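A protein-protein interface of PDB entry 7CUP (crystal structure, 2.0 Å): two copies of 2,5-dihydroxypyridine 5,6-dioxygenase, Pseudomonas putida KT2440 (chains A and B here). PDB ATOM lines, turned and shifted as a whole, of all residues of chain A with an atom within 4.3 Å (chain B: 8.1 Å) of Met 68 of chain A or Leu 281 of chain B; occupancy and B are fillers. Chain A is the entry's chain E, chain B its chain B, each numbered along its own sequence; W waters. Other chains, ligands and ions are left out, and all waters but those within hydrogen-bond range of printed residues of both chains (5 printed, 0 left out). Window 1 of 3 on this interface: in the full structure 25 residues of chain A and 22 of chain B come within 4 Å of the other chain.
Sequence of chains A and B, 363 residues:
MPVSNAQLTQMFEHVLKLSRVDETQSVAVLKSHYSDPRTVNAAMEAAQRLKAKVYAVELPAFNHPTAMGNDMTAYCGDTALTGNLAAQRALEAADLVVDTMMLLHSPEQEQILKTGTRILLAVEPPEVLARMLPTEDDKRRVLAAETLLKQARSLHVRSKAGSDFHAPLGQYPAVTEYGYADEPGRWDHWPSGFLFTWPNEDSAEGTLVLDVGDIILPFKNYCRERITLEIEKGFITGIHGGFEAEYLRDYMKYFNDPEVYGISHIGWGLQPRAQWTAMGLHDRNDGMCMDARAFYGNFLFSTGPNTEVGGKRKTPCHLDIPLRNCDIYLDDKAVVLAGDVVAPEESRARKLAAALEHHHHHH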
ATOM      1  N   THR A  66     -16.712 -13.402  15.094  1.00  0.00           N
ATOM      2  CA  THR A  66     -16.187 -12.033  14.848  1.00  0.00           C
ATOM      3  C   THR A  66     -16.510 -11.554  13.428  1.00  0.00           C
ATOM      4  O   THR A  66     -16.167 -10.382  13.127  1.00  0.00           O
ATOM      5  CB  THR A  66     -14.677 -11.941  15.100  1.00  0.00           C
ATOM      6  OG1 THR A  66     -13.986 -12.722  14.129  1.00  0.00           O
ATOM      7  CG2 THR A  66     -14.305 -12.377  16.508  1.00  0.00           C
ATOM      8  N   ALA A  67     -17.135 -12.372  12.576  1.00  0.00           N
ATOM      9  CA  ALA A  67     -17.472 -11.912  11.210  1.00  0.00           C
ATOM     10  C   ALA A  67     -18.608 -10.881  11.317  1.00  0.00           C
ATOM     11  O   ALA A  67     -19.490 -11.020  12.236  1.00  0.00           O
ATOM     12  CB  ALA A  67     -17.803 -13.068  10.292  1.00  0.00           C
ATOM     13  N   MET A  68     -18.550  -9.848  10.478  1.00  0.00           N
ATOM     14  CA  MET A  68     -19.590  -8.795  10.361  1.00  0.00           C
ATOM     15  C   MET A  68     -20.312  -8.859   8.996  1.00  0.00           C
ATOM     16  O   MET A  68     -19.659  -9.058   7.964  1.00  0.00           O
ATOM     17  CB  MET A  68     -18.962  -7.419  10.545  1.00  0.00           C
ATOM     18  CG  MET A  68     -18.262  -7.272  11.878  1.00  0.00           C
ATOM     19  SD  MET A  68     -17.830  -5.564  12.142  1.00  0.00           S
ATOM     20  CE  MET A  68     -16.369  -5.406  11.124  1.00  0.00           C
ATOM     21  N   GLY A  69     -21.626  -8.649   9.001  1.00  0.00           N
ATOM     22  CA  GLY A  69     -22.470  -8.735   7.797  1.00  0.00           C
ATOM     23  C   GLY A  69     -22.841 -10.180   7.468  1.00  0.00           C
ATOM     24  O   GLY A  69     -22.343 -11.096   8.149  1.00  0.00           O
ATOM     25  N   PRO A 218     -16.700  -7.205   0.396  1.00  0.00           N
ATOM     26  CA  PRO A 218     -18.152  -7.307   0.517  1.00  0.00           C
ATOM     27  C   PRO A 218     -18.905  -6.057   0.958  1.00  0.00           C
ATOM     28  O   PRO A 218     -20.081  -6.206   1.339  1.00  0.00           O
ATOM     29  CB  PRO A 218     -18.272  -8.378   1.616  1.00  0.00           C
ATOM     30  CG  PRO A 218     -17.126  -8.047   2.552  1.00  0.00           C
ATOM     31  CD  PRO A 218     -16.007  -7.569   1.642  1.00  0.00           C
ATOM     32  N   PHE A 219     -18.284  -4.877   0.893  1.00  0.00           N
ATOM     33  CA  PHE A 219     -18.952  -3.609   1.261  1.00  0.00           C
ATOM     34  C   PHE A 219     -20.115  -3.391   0.286  1.00  0.00           C
ATOM     35  O   PHE A 219     -21.158  -2.866   0.697  1.00  0.00           O
ATOM     36  CB  PHE A 219     -18.012  -2.399   1.243  1.00  0.00           C
ATOM     37  CG  PHE A 219     -16.749  -2.494   2.054  1.00  0.00           C
ATOM     38  CD1 PHE A 219     -16.553  -3.502   2.980  1.00  0.00           C
ATOM     39  CD2 PHE A 219     -15.773  -1.521   1.922  1.00  0.00           C
ATOM     40  CE1 PHE A 219     -15.386  -3.563   3.717  1.00  0.00           C
ATOM     41  CE2 PHE A 219     -14.622  -1.566   2.683  1.00  0.00           C
ATOM     42  CZ  PHE A 219     -14.421  -2.597   3.564  1.00  0.00           C
ATOM     43  N   TYR A 247     -12.613   4.140   6.162  1.00  0.00           N
ATOM     44  CA  TYR A 247     -13.517   3.002   6.428  1.00  0.00           C
ATOM     45  C   TYR A 247     -12.750   1.713   6.124  1.00  0.00           C
ATOM     46  O   TYR A 247     -12.676   0.825   6.989  1.00  0.00           O
ATOM     47  CB  TYR A 247     -14.817   3.142   5.629  1.00  0.00           C
ATOM     48  CG  TYR A 247     -15.802   2.024   5.855  1.00  0.00           C
ATOM     49  CD1 TYR A 247     -15.662   0.814   5.208  1.00  0.00           C
ATOM     50  CD2 TYR A 247     -16.880   2.178   6.716  1.00  0.00           C
ATOM     51  CE1 TYR A 247     -16.565  -0.219   5.409  1.00  0.00           C
ATOM     52  CE2 TYR A 247     -17.779   1.149   6.939  1.00  0.00           C
ATOM     53  CZ  TYR A 247     -17.648  -0.040   6.253  1.00  0.00           C
ATOM     54  OH  TYR A 247     -18.541  -1.058   6.438  1.00  0.00           O
ATOM     55  N   TYR A 251     -11.717  -1.177   8.726  1.00  0.00           N
ATOM     56  CA  TYR A 251     -12.238  -2.553   8.520  1.00  0.00           C
ATOM     57  C   TYR A 251     -11.085  -3.556   8.540  1.00  0.00           C
ATOM     58  O   TYR A 251     -11.197  -4.572   9.234  1.00  0.00           O
ATOM     59  CB  TYR A 251     -12.995  -2.670   7.201  1.00  0.00           C
ATOM     60  CG  TYR A 251     -13.542  -4.049   6.946  1.00  0.00           C
ATOM     61  CD1 TYR A 251     -14.669  -4.501   7.612  1.00  0.00           C
ATOM     62  CD2 TYR A 251     -12.944  -4.911   6.040  1.00  0.00           C
ATOM     63  CE1 TYR A 251     -15.201  -5.761   7.369  1.00  0.00           C
ATOM     64  CE2 TYR A 251     -13.450  -6.183   5.801  1.00  0.00           C
ATOM     65  CZ  TYR A 251     -14.588  -6.599   6.461  1.00  0.00           C
ATOM     66  OH  TYR A 251     -15.110  -7.826   6.209  1.00  0.00           O
ATOM     67  N   TYR A 254      -9.335  -4.111  12.036  1.00  0.00           N
ATOM     68  CA  TYR A 254     -10.189  -4.896  12.968  1.00  0.00           C
ATOM     69  C   TYR A 254      -9.701  -6.340  13.064  1.00  0.00           C
ATOM     70  O   TYR A 254      -9.827  -6.937  14.140  1.00  0.00           O
ATOM     71  CB  TYR A 254     -11.635  -4.901  12.478  1.00  0.00           C
ATOM     72  CG  TYR A 254     -12.589  -5.911  13.082  1.00  0.00           C
ATOM     73  CD1 TYR A 254     -13.114  -5.706  14.344  1.00  0.00           C
ATOM     74  CD2 TYR A 254     -13.056  -6.996  12.335  1.00  0.00           C
ATOM     75  CE1 TYR A 254     -14.043  -6.576  14.884  1.00  0.00           C
ATOM     76  CE2 TYR A 254     -14.020  -7.853  12.845  1.00  0.00           C
ATOM     77  CZ  TYR A 254     -14.497  -7.651  14.137  1.00  0.00           C
ATOM     78  OH  TYR A 254     -15.455  -8.459  14.675  1.00  0.00           O
ATOM     79  N   ARG A 284     -27.860  -5.457  -0.201  1.00  0.00           N
ATOM     80  CA  ARG A 284     -26.597  -6.186   0.099  1.00  0.00           C
ATOM     81  C   ARG A 284     -26.907  -7.661   0.323  1.00  0.00           C
ATOM     82  O   ARG A 284     -26.109  -8.504  -0.158  1.00  0.00           O
ATOM     83  CB  ARG A 284     -25.945  -5.636   1.368  1.00  0.00           C
ATOM     84  CG  ARG A 284     -25.500  -4.191   1.230  1.00  0.00           C
ATOM     85  CD  ARG A 284     -24.486  -3.828   2.301  1.00  0.00           C
ATOM     86  NE  ARG A 284     -23.909  -2.540   1.984  1.00  0.00           N
ATOM     87  CZ  ARG A 284     -24.459  -1.378   2.281  1.00  0.00           C
ATOM     88  NH1 ARG A 284     -25.601  -1.311   2.942  1.00  0.00           N
ATOM     89  NH2 ARG A 284     -23.835  -0.271   1.958  1.00  0.00           N
ATOM     90  N   GLU B 127     -26.575 -13.639  14.284  1.00  0.00           N
ATOM     91  CA  GLU B 127     -25.121 -13.437  14.048  1.00  0.00           C
ATOM     92  C   GLU B 127     -24.616 -12.227  14.883  1.00  0.00           C
ATOM     93  O   GLU B 127     -23.481 -12.271  15.413  1.00  0.00           O
ATOM     94  CB  GLU B 127     -24.823 -13.303  12.553  1.00  0.00           C
ATOM     95  CG  GLU B 127     -25.099 -14.609  11.792  1.00  0.00           C
ATOM     96  CD  GLU B 127     -26.573 -14.977  11.653  1.00  0.00           C
ATOM     97  OE1 GLU B 127     -27.443 -14.009  11.670  1.00  0.00           O
ATOM     98  OE2 GLU B 127     -26.871 -16.233  11.569  1.00  0.00           O
ATOM     99  N   VAL B 128     -25.394 -11.149  14.965  1.00  0.00           N
ATOM    100  CA  VAL B 128     -25.071  -9.948  15.799  1.00  0.00           C
ATOM    101  C   VAL B 128     -25.156 -10.364  17.278  1.00  0.00           C
ATOM    102  O   VAL B 128     -24.271  -9.976  18.052  1.00  0.00           O
ATOM    103  CB  VAL B 128     -26.021  -8.792  15.466  1.00  0.00           C
ATOM    104  CG1 VAL B 128     -25.816  -7.596  16.374  1.00  0.00           C
ATOM    105  CG2 VAL B 128     -25.928  -8.395  13.998  1.00  0.00           C
ATOM    106  N   ARG B 131     -21.921 -12.112  17.980  1.00  0.00           N
ATOM    107  CA  ARG B 131     -20.685 -11.310  17.892  1.00  0.00           C
ATOM    108  C   ARG B 131     -20.507 -10.550  19.216  1.00  0.00           C
ATOM    109  O   ARG B 131     -19.331 -10.327  19.648  1.00  0.00           O
ATOM    110  CB  ARG B 131     -20.723 -10.338  16.722  1.00  0.00           C
ATOM    111  CG  ARG B 131     -19.425  -9.565  16.527  1.00  0.00           C
ATOM    112  CD  ARG B 131     -19.309  -9.105  15.098  1.00  0.00           C
ATOM    113  NE  ARG B 131     -20.504  -8.489  14.530  1.00  0.00           N
ATOM    114  CZ  ARG B 131     -20.925  -7.269  14.793  1.00  0.00           C
ATOM    115  NH1 ARG B 131     -20.298  -6.517  15.681  1.00  0.00           N
ATOM    116  NH2 ARG B 131     -21.983  -6.787  14.167  1.00  0.00           N
ATOM    117  N   TYR B 222     -23.699   6.874   6.812  1.00  0.00           N
ATOM    118  CA  TYR B 222     -22.461   7.572   7.192  1.00  0.00           C
ATOM    119  C   TYR B 222     -22.510   8.931   6.515  1.00  0.00           C
ATOM    120  O   TYR B 222     -22.663   8.958   5.295  1.00  0.00           O
ATOM    121  CB  TYR B 222     -21.256   6.764   6.717  1.00  0.00           C
ATOM    122  CG  TYR B 222     -21.107   5.401   7.340  1.00  0.00           C
ATOM    123  CD1 TYR B 222     -20.423   5.240   8.525  1.00  0.00           C
ATOM    124  CD2 TYR B 222     -21.565   4.261   6.702  1.00  0.00           C
ATOM    125  CE1 TYR B 222     -20.202   3.990   9.078  1.00  0.00           C
ATOM    126  CE2 TYR B 222     -21.408   3.010   7.267  1.00  0.00           C
ATOM    127  CZ  TYR B 222     -20.703   2.867   8.449  1.00  0.00           C
ATOM    128  OH  TYR B 222     -20.522   1.635   9.015  1.00  0.00           O
ATOM    129  N   ARG B 273     -16.514  -5.024  20.882  1.00  0.00           N
ATOM    130  CA  ARG B 273     -16.980  -6.064  19.912  1.00  0.00           C
ATOM    131  C   ARG B 273     -18.032  -5.452  18.947  1.00  0.00           C
ATOM    132  O   ARG B 273     -18.361  -6.063  17.901  1.00  0.00           O
ATOM    133  CB  ARG B 273     -17.468  -7.303  20.666  1.00  0.00           C
ATOM    134  CG  ARG B 273     -16.339  -8.134  21.281  1.00  0.00           C
ATOM    135  CD  ARG B 273     -16.838  -9.373  22.010  1.00  0.00           C
ATOM    136  NE  ARG B 273     -17.619  -8.984  23.173  1.00  0.00           N
ATOM    137  CZ  ARG B 273     -18.581  -9.702  23.734  1.00  0.00           C
ATOM    138  NH1 ARG B 273     -18.928 -10.865  23.202  1.00  0.00           N
ATOM    139  NH2 ARG B 273     -19.244  -9.208  24.774  1.00  0.00           N
ATOM    140  N   ALA B 274     -18.530  -4.267  19.266  1.00  0.00           N
ATOM    141  CA  ALA B 274     -19.340  -3.450  18.335  1.00  0.00           C
ATOM    142  C   ALA B 274     -18.349  -2.675  17.472  1.00  0.00           C
ATOM    143  O   ALA B 274     -17.250  -2.358  17.980  1.00  0.00           O
ATOM    144  CB  ALA B 274     -20.249  -2.519  19.069  1.00  0.00           C
ATOM    145  N   GLN B 275     -18.718  -2.387  16.234  1.00  0.00           N
ATOM    146  CA  GLN B 275     -17.808  -1.781  15.231  1.00  0.00           C
ATOM    147  C   GLN B 275     -18.564  -0.717  14.449  1.00  0.00           C
ATOM    148  O   GLN B 275     -19.716  -0.962  13.990  1.00  0.00           O
ATOM    149  CB  GLN B 275     -17.259  -2.880  14.333  1.00  0.00           C
ATOM    150  CG  GLN B 275     -16.335  -3.839  15.052  1.00  0.00           C
ATOM    151  CD  GLN B 275     -15.039  -3.170  15.430  1.00  0.00           C
ATOM    152  OE1 GLN B 275     -14.397  -2.522  14.617  1.00  0.00           O
ATOM    153  NE2 GLN B 275     -14.626  -3.368  16.663  1.00  0.00           N
ATOM    154  N   TRP B 276     -17.939   0.453  14.393  1.00  0.00           N
ATOM    155  CA  TRP B 276     -18.389   1.614  13.606  1.00  0.00           C
ATOM    156  C   TRP B 276     -18.587   1.193  12.158  1.00  0.00           C
ATOM    157  O   TRP B 276     -19.482   1.722  11.534  1.00  0.00           O
ATOM    158  CB  TRP B 276     -17.366   2.736  13.764  1.00  0.00           C
ATOM    159  CG  TRP B 276     -17.497   3.839  12.776  1.00  0.00           C
ATOM    160  CD1 TRP B 276     -18.455   4.807  12.765  1.00  0.00           C
ATOM    161  CD2 TRP B 276     -16.631   4.096  11.655  1.00  0.00           C
ATOM    162  NE1 TRP B 276     -18.261   5.642  11.694  1.00  0.00           N
ATOM    163  CE2 TRP B 276     -17.146   5.242  11.002  1.00  0.00           C
ATOM    164  CE3 TRP B 276     -15.458   3.512  11.170  1.00  0.00           C
ATOM    165  CZ2 TRP B 276     -16.548   5.798   9.873  1.00  0.00           C
ATOM    166  CZ3 TRP B 276     -14.852   4.071  10.063  1.00  0.00           C
ATOM    167  CH2 TRP B 276     -15.401   5.185   9.414  1.00  0.00           C
ATOM    168  N   THR B 277     -17.779   0.255  11.658  1.00  0.00           N
ATOM    169  CA  THR B 277     -17.840  -0.204  10.239  1.00  0.00           C
ATOM    170  C   THR B 277     -19.027  -1.161  10.019  1.00  0.00           C
ATOM    171  O   THR B 277     -19.374  -1.383   8.848  1.00  0.00           O
ATOM    172  CB  THR B 277     -16.550  -0.910   9.776  1.00  0.00           C
ATOM    173  OG1 THR B 277     -16.295  -1.980  10.677  1.00  0.00           O
ATOM    174  CG2 THR B 277     -15.350   0.005   9.662  1.00  0.00           C
ATOM    175  N   ALA B 278     -19.618  -1.748  11.053  1.00  0.00           N
ATOM    176  CA  ALA B 278     -20.590  -2.861  10.875  1.00  0.00           C
ATOM    177  C   ALA B 278     -21.797  -2.416  10.031  1.00  0.00           C
ATOM    178  O   ALA B 278     -22.274  -3.221   9.193  1.00  0.00           O
ATOM    179  CB  ALA B 278     -21.061  -3.412  12.190  1.00  0.00           C
ATOM    180  N   MET B 279     -22.294  -1.202  10.244  1.00  0.00           N
ATOM    181  CA  MET B 279     -23.562  -0.730   9.629  1.00  0.00           C
ATOM    182  C   MET B 279     -23.423  -0.801   8.101  1.00  0.00           C
ATOM    183  O   MET B 279     -24.403  -1.182   7.444  1.00  0.00           O
ATOM    184  CB  MET B 279     -23.858   0.700  10.092  1.00  0.00           C
ATOM    185  CG  MET B 279     -25.162   1.259   9.598  1.00  0.00           C
ATOM    186  SD  MET B 279     -25.500   2.943  10.252  1.00  0.00           S
ATOM    187  CE  MET B 279     -24.304   3.910   9.328  1.00  0.00           C
ATOM    188  N   GLY B 280     -22.227  -0.498   7.570  1.00  0.00           N
ATOM    189  CA  GLY B 280     -21.902  -0.492   6.127  1.00  0.00           C
ATOM    190  C   GLY B 280     -22.002  -1.864   5.462  1.00  0.00           C
ATOM    191  O   GLY B 280     -21.987  -1.924   4.232  1.00  0.00           O
ATOM    192  N   LEU B 281     -22.098  -2.936   6.241  1.00  0.00           N
ATOM    193  CA  LEU B 281     -22.087  -4.316   5.722  1.00  0.00           C
ATOM    194  C   LEU B 281     -23.505  -4.878   5.746  1.00  0.00           C
ATOM    195  O   LEU B 281     -23.670  -6.034   5.316  1.00  0.00           O
ATOM    196  CB  LEU B 281     -21.129  -5.144   6.585  1.00  0.00           C
ATOM    197  CG  LEU B 281     -19.655  -4.836   6.346  1.00  0.00           C
ATOM    198  CD1 LEU B 281     -18.835  -5.005   7.609  1.00  0.00           C
ATOM    199  CD2 LEU B 281     -19.103  -5.721   5.239  1.00  0.00           C
ATOM    200  N   HIS B 282     -24.476  -4.102   6.250  1.00  0.00           N
ATOM    201  CA  HIS B 282     -25.855  -4.569   6.537  1.00  0.00           C
ATOM    202  C   HIS B 282     -26.884  -3.780   5.699  1.00  0.00           C
ATOM    203  O   HIS B 282     -26.547  -2.718   5.135  1.00  0.00           O
ATOM    204  CB  HIS B 282     -26.123  -4.485   8.050  1.00  0.00           C
ATOM    205  CG  HIS B 282     -25.612  -5.636   8.849  1.00  0.00           C
ATOM    206  ND1 HIS B 282     -26.307  -6.828   8.934  1.00  0.00           N
ATOM    207  CD2 HIS B 282     -24.482  -5.782   9.590  1.00  0.00           C
ATOM    208  CE1 HIS B 282     -25.655  -7.662   9.724  1.00  0.00           C
ATOM    209  NE2 HIS B 282     -24.524  -7.031  10.146  1.00  0.00           N
ATOM    210  N   ASP B 283     -28.088  -4.342   5.554  1.00  0.00           N
ATOM    211  CA  ASP B 283     -29.234  -3.643   4.943  1.00  0.00           C
ATOM    212  C   ASP B 283     -29.976  -2.997   6.108  1.00  0.00           C
ATOM    213  O   ASP B 283     -29.816  -3.482   7.259  1.00  0.00           O
ATOM    214  CB  ASP B 283     -30.083  -4.607   4.107  1.00  0.00           C
ATOM    215  CG  ASP B 283     -29.460  -4.979   2.771  1.00  0.00           C
ATOM    216  OD1 ASP B 283     -28.789  -4.105   2.151  1.00  0.00           O
ATOM    217  OD2 ASP B 283     -29.608  -6.152   2.380  1.00  0.00           O
ATOM    218  N   ARG B 284     -30.758  -1.958   5.849  1.00  0.00           N
ATOM    219  CA  ARG B 284     -31.465  -1.213   6.923  1.00  0.00           C
ATOM    220  C   ARG B 284     -32.402  -2.116   7.725  1.00  0.00           C
ATOM    221  O   ARG B 284     -32.459  -1.968   8.955  1.00  0.00           O
ATOM    222  CB  ARG B 284     -32.262  -0.068   6.320  1.00  0.00           C
ATOM    223  CG  ARG B 284     -31.363   0.983   5.729  1.00  0.00           C
ATOM    224  CD  ARG B 284     -32.175   2.234   5.601  1.00  0.00           C
ATOM    225  NE  ARG B 284     -31.257   3.269   5.217  1.00  0.00           N
ATOM    226  CZ  ARG B 284     -30.873   3.512   3.974  1.00  0.00           C
ATOM    227  NH1 ARG B 284     -31.350   2.790   2.984  1.00  0.00           N
ATOM    228  NH2 ARG B 284     -30.011   4.483   3.742  1.00  0.00           N
ATOM    229  N   ASP B 286     -32.118  -5.091   8.559  1.00  0.00           N
ATOM    230  CA  ASP B 286     -31.437  -6.202   9.280  1.00  0.00           C
ATOM    231  C   ASP B 286     -31.686  -6.039  10.781  1.00  0.00           C
ATOM    232  O   ASP B 286     -31.782  -7.043  11.477  1.00  0.00           O
ATOM    233  CB  ASP B 286     -29.953  -6.332   8.948  1.00  0.00           C
ATOM    234  CG  ASP B 286     -29.672  -6.808   7.536  1.00  0.00           C
ATOM    235  OD1 ASP B 286     -28.505  -6.756   7.129  1.00  0.00           O
ATOM    236  OD2 ASP B 286     -30.637  -7.167   6.846  1.00  0.00           O
ATOM    237  N   ASP B 291     -24.506  -1.883  16.882  1.00  0.00           N
ATOM    238  CA  ASP B 291     -23.073  -1.565  16.632  1.00  0.00           C
ATOM    239  C   ASP B 291     -22.819  -0.043  16.673  1.00  0.00           C
ATOM    240  O   ASP B 291     -21.817   0.421  17.309  1.00  0.00           O
ATOM    241  CB  ASP B 291     -22.620  -2.125  15.293  1.00  0.00           C
ATOM    242  CG  ASP B 291     -22.223  -3.573  15.357  1.00  0.00           C
ATOM    243  OD1 ASP B 291     -21.069  -3.826  15.759  1.00  0.00           O
ATOM    244  OD2 ASP B 291     -23.064  -4.444  14.994  1.00  0.00           O
HETATM  245  O   HOH W   1     -22.659  -8.012  11.749  1.00  0.00           O
HETATM  246  O   HOH W   2     -22.212  -7.377   3.012  1.00  0.00           O
HETATM  247  O   HOH W   3     -24.013 -10.428  10.607  1.00  0.00           O
HETATM  248  O   HOH W   4     -21.980 -10.452  13.166  1.00  0.00           O
HETATM  249  O   HOH W   5     -16.320  -8.079  17.236  1.00  0.00           O
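The guanidinium group of Arg 131 of chain B sits at hydrogen-bond distance from the backbone carbonyl oxygen of Arg 273 of chain B, 3.0 Å away. The side-chain carboxylate of Asp 291 of chain B is in salt-bridge range of the guanidinium group of Arg 131 of chain B (2.7 Å). The side-chain hydroxyl (OH) of Tyr 222 of chain B sits at hydrogen-bond distance from the backbone NH (N) of Gly 280 of chain B, at 3.1 Å. The backbone NH of Gln 275 of chain B lies within hydrogen-bond range of the side-chain carboxylate of Asp 291 of chain B. OH of Tyr 254 of chain A is in hydrogen-bond range of O of Thr 66 of chain A (2.6 Å). The guanidinium group of Arg 284 of chain A is in hydrogen-bond range of the backbone carbonyl oxygen of Phe 219 of chain A, at 3.1 Å.
Ala 67 of chain A touches just one residue of chain B: Arg 131 (3.4 Å). Met 68 of chain A touches just these residues of chain B: Arg 131, Gln 275, Thr 277, Ala 278 and Leu 281. Of chain B, only Leu 281 and His 282 come within 4 Å of Gly 69 of chain A. Pro 218 of chain A touches none of the printed residues of chain B. Of the printed residues of chain B, Tyr 251 of chain A touches Thr 277 (3.9 Å) and Leu 281 (3.7 Å). Glu 127 of chain B touches none of the printed residues of chain A. Of the printed residues of chain A, Arg 131 of chain B touches Thr 66 (3.9 Å), Ala 67 (3.4 Å), Met 68 (3.7 Å) and Tyr 254 (3.9 Å). Of the printed residues of chain A, Gln 275 of chain B touches Met 68 and Tyr 254. Of the printed residues of chain A, Ala 278 of chain B touches Met 68 (3.9 Å). Leu 281 of chain B touches five residues of chain A. The nearest residue of chain B that does not touch Met 68 of chain A is His 282 of chain B (4.7 Å).
Water W1 lies within hydrogen-bond range of a ring nitrogen (NE2) of His 282 of chain B, the guanidinium group of Arg 131 of chain B and the backbone NH of Gly 69 of chain A. Water W4 lies within hydrogen-bond range of O of Ala 67 of chain A (2.7 Å), NE of Arg 131 of chain B (2.8 Å) and O of Glu 127 of chain B (3.3 Å). Water W5 lies within hydrogen-bond range of the side-chain hydroxyl of Tyr 254 of chain A (2.7 Å) and the backbone carbonyl oxygen of Arg 273 of chain B (2.9 Å). Water W2 bridges the backbone carbonyl oxygen of Pro 218 of chain A (3.0 Å) and the backbone carbonyl oxygen of Leu 281 of chain B (3.0 Å). Water W3 lies within hydrogen-bond range of the backbone carbonyl oxygen (O) of Gly 69 of chain A (3.0 Å) and a ring nitrogen (NE2) of His 282 of chain B (3.5 Å).
Arg 131 of chain B touches Thr 66 of chain A. CG of Met 68 of chain A touches NE of Arg 131 of chain B, at 3.7 Å. Gln 275 of chain B touches Met 68 of chain A (CB to SD, 3.5 Å). Met 68 of chain A touches Leu 281 of chain B. His 282 of chain B touches Gly 69 of chain A (NE2 to N, 3.5 Å). Tyr 247 of chain A touches Gly 280 of chain B. OH of Tyr 247 of chain A touches CG of Leu 281 of chain B, 3.9 Å away. CE1 of Tyr 251 of chain A touches CD1 of Leu 281 of chain B, 3.7 Å away. Arg 131 of chain B touches Tyr 254 of chain A (CD to OH, 3.9 Å). Arg 284 of chain A touches Leu 281 of chain B.
The backbone carbonyl oxygen (O) of Thr 277 of chain B sits at hydrogen-bond distance from the side-chain hydroxyl (OH) of Tyr 247 of chain A, 2.6 Å away. The backbone carbonyl oxygen (O) of Gly 280 of chain B is in hydrogen-bond range of the guanidinium group (NE) of Arg 284 of chain A. The guanidinium group (NH1) of Arg 284 of chain A is in hydrogen-bond range of the backbone carbonyl oxygen (O) of His 282 of chain B (2.8 Å). The side-chain carboxylate (OD1) of Asp 283 of chain B is in hydrogen-bond range of the backbone NH (N) of Arg 284 of chain A, 2.9 Å away.
Of the 18 printed residues of chain B, 9 touch a printed residue of chain A. Hydrophobic or aromatic side chains of chain B that line the printed part of chain A: Tyr 222, Ala 278, Leu 281 and His 282. Among the printed residues, 22 pairs touch across the chains.
Position printed for both chains: 284. Of the 22 pairs that touch across the chains among the printed residues, none has its exchanged pair printed and touching as well.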
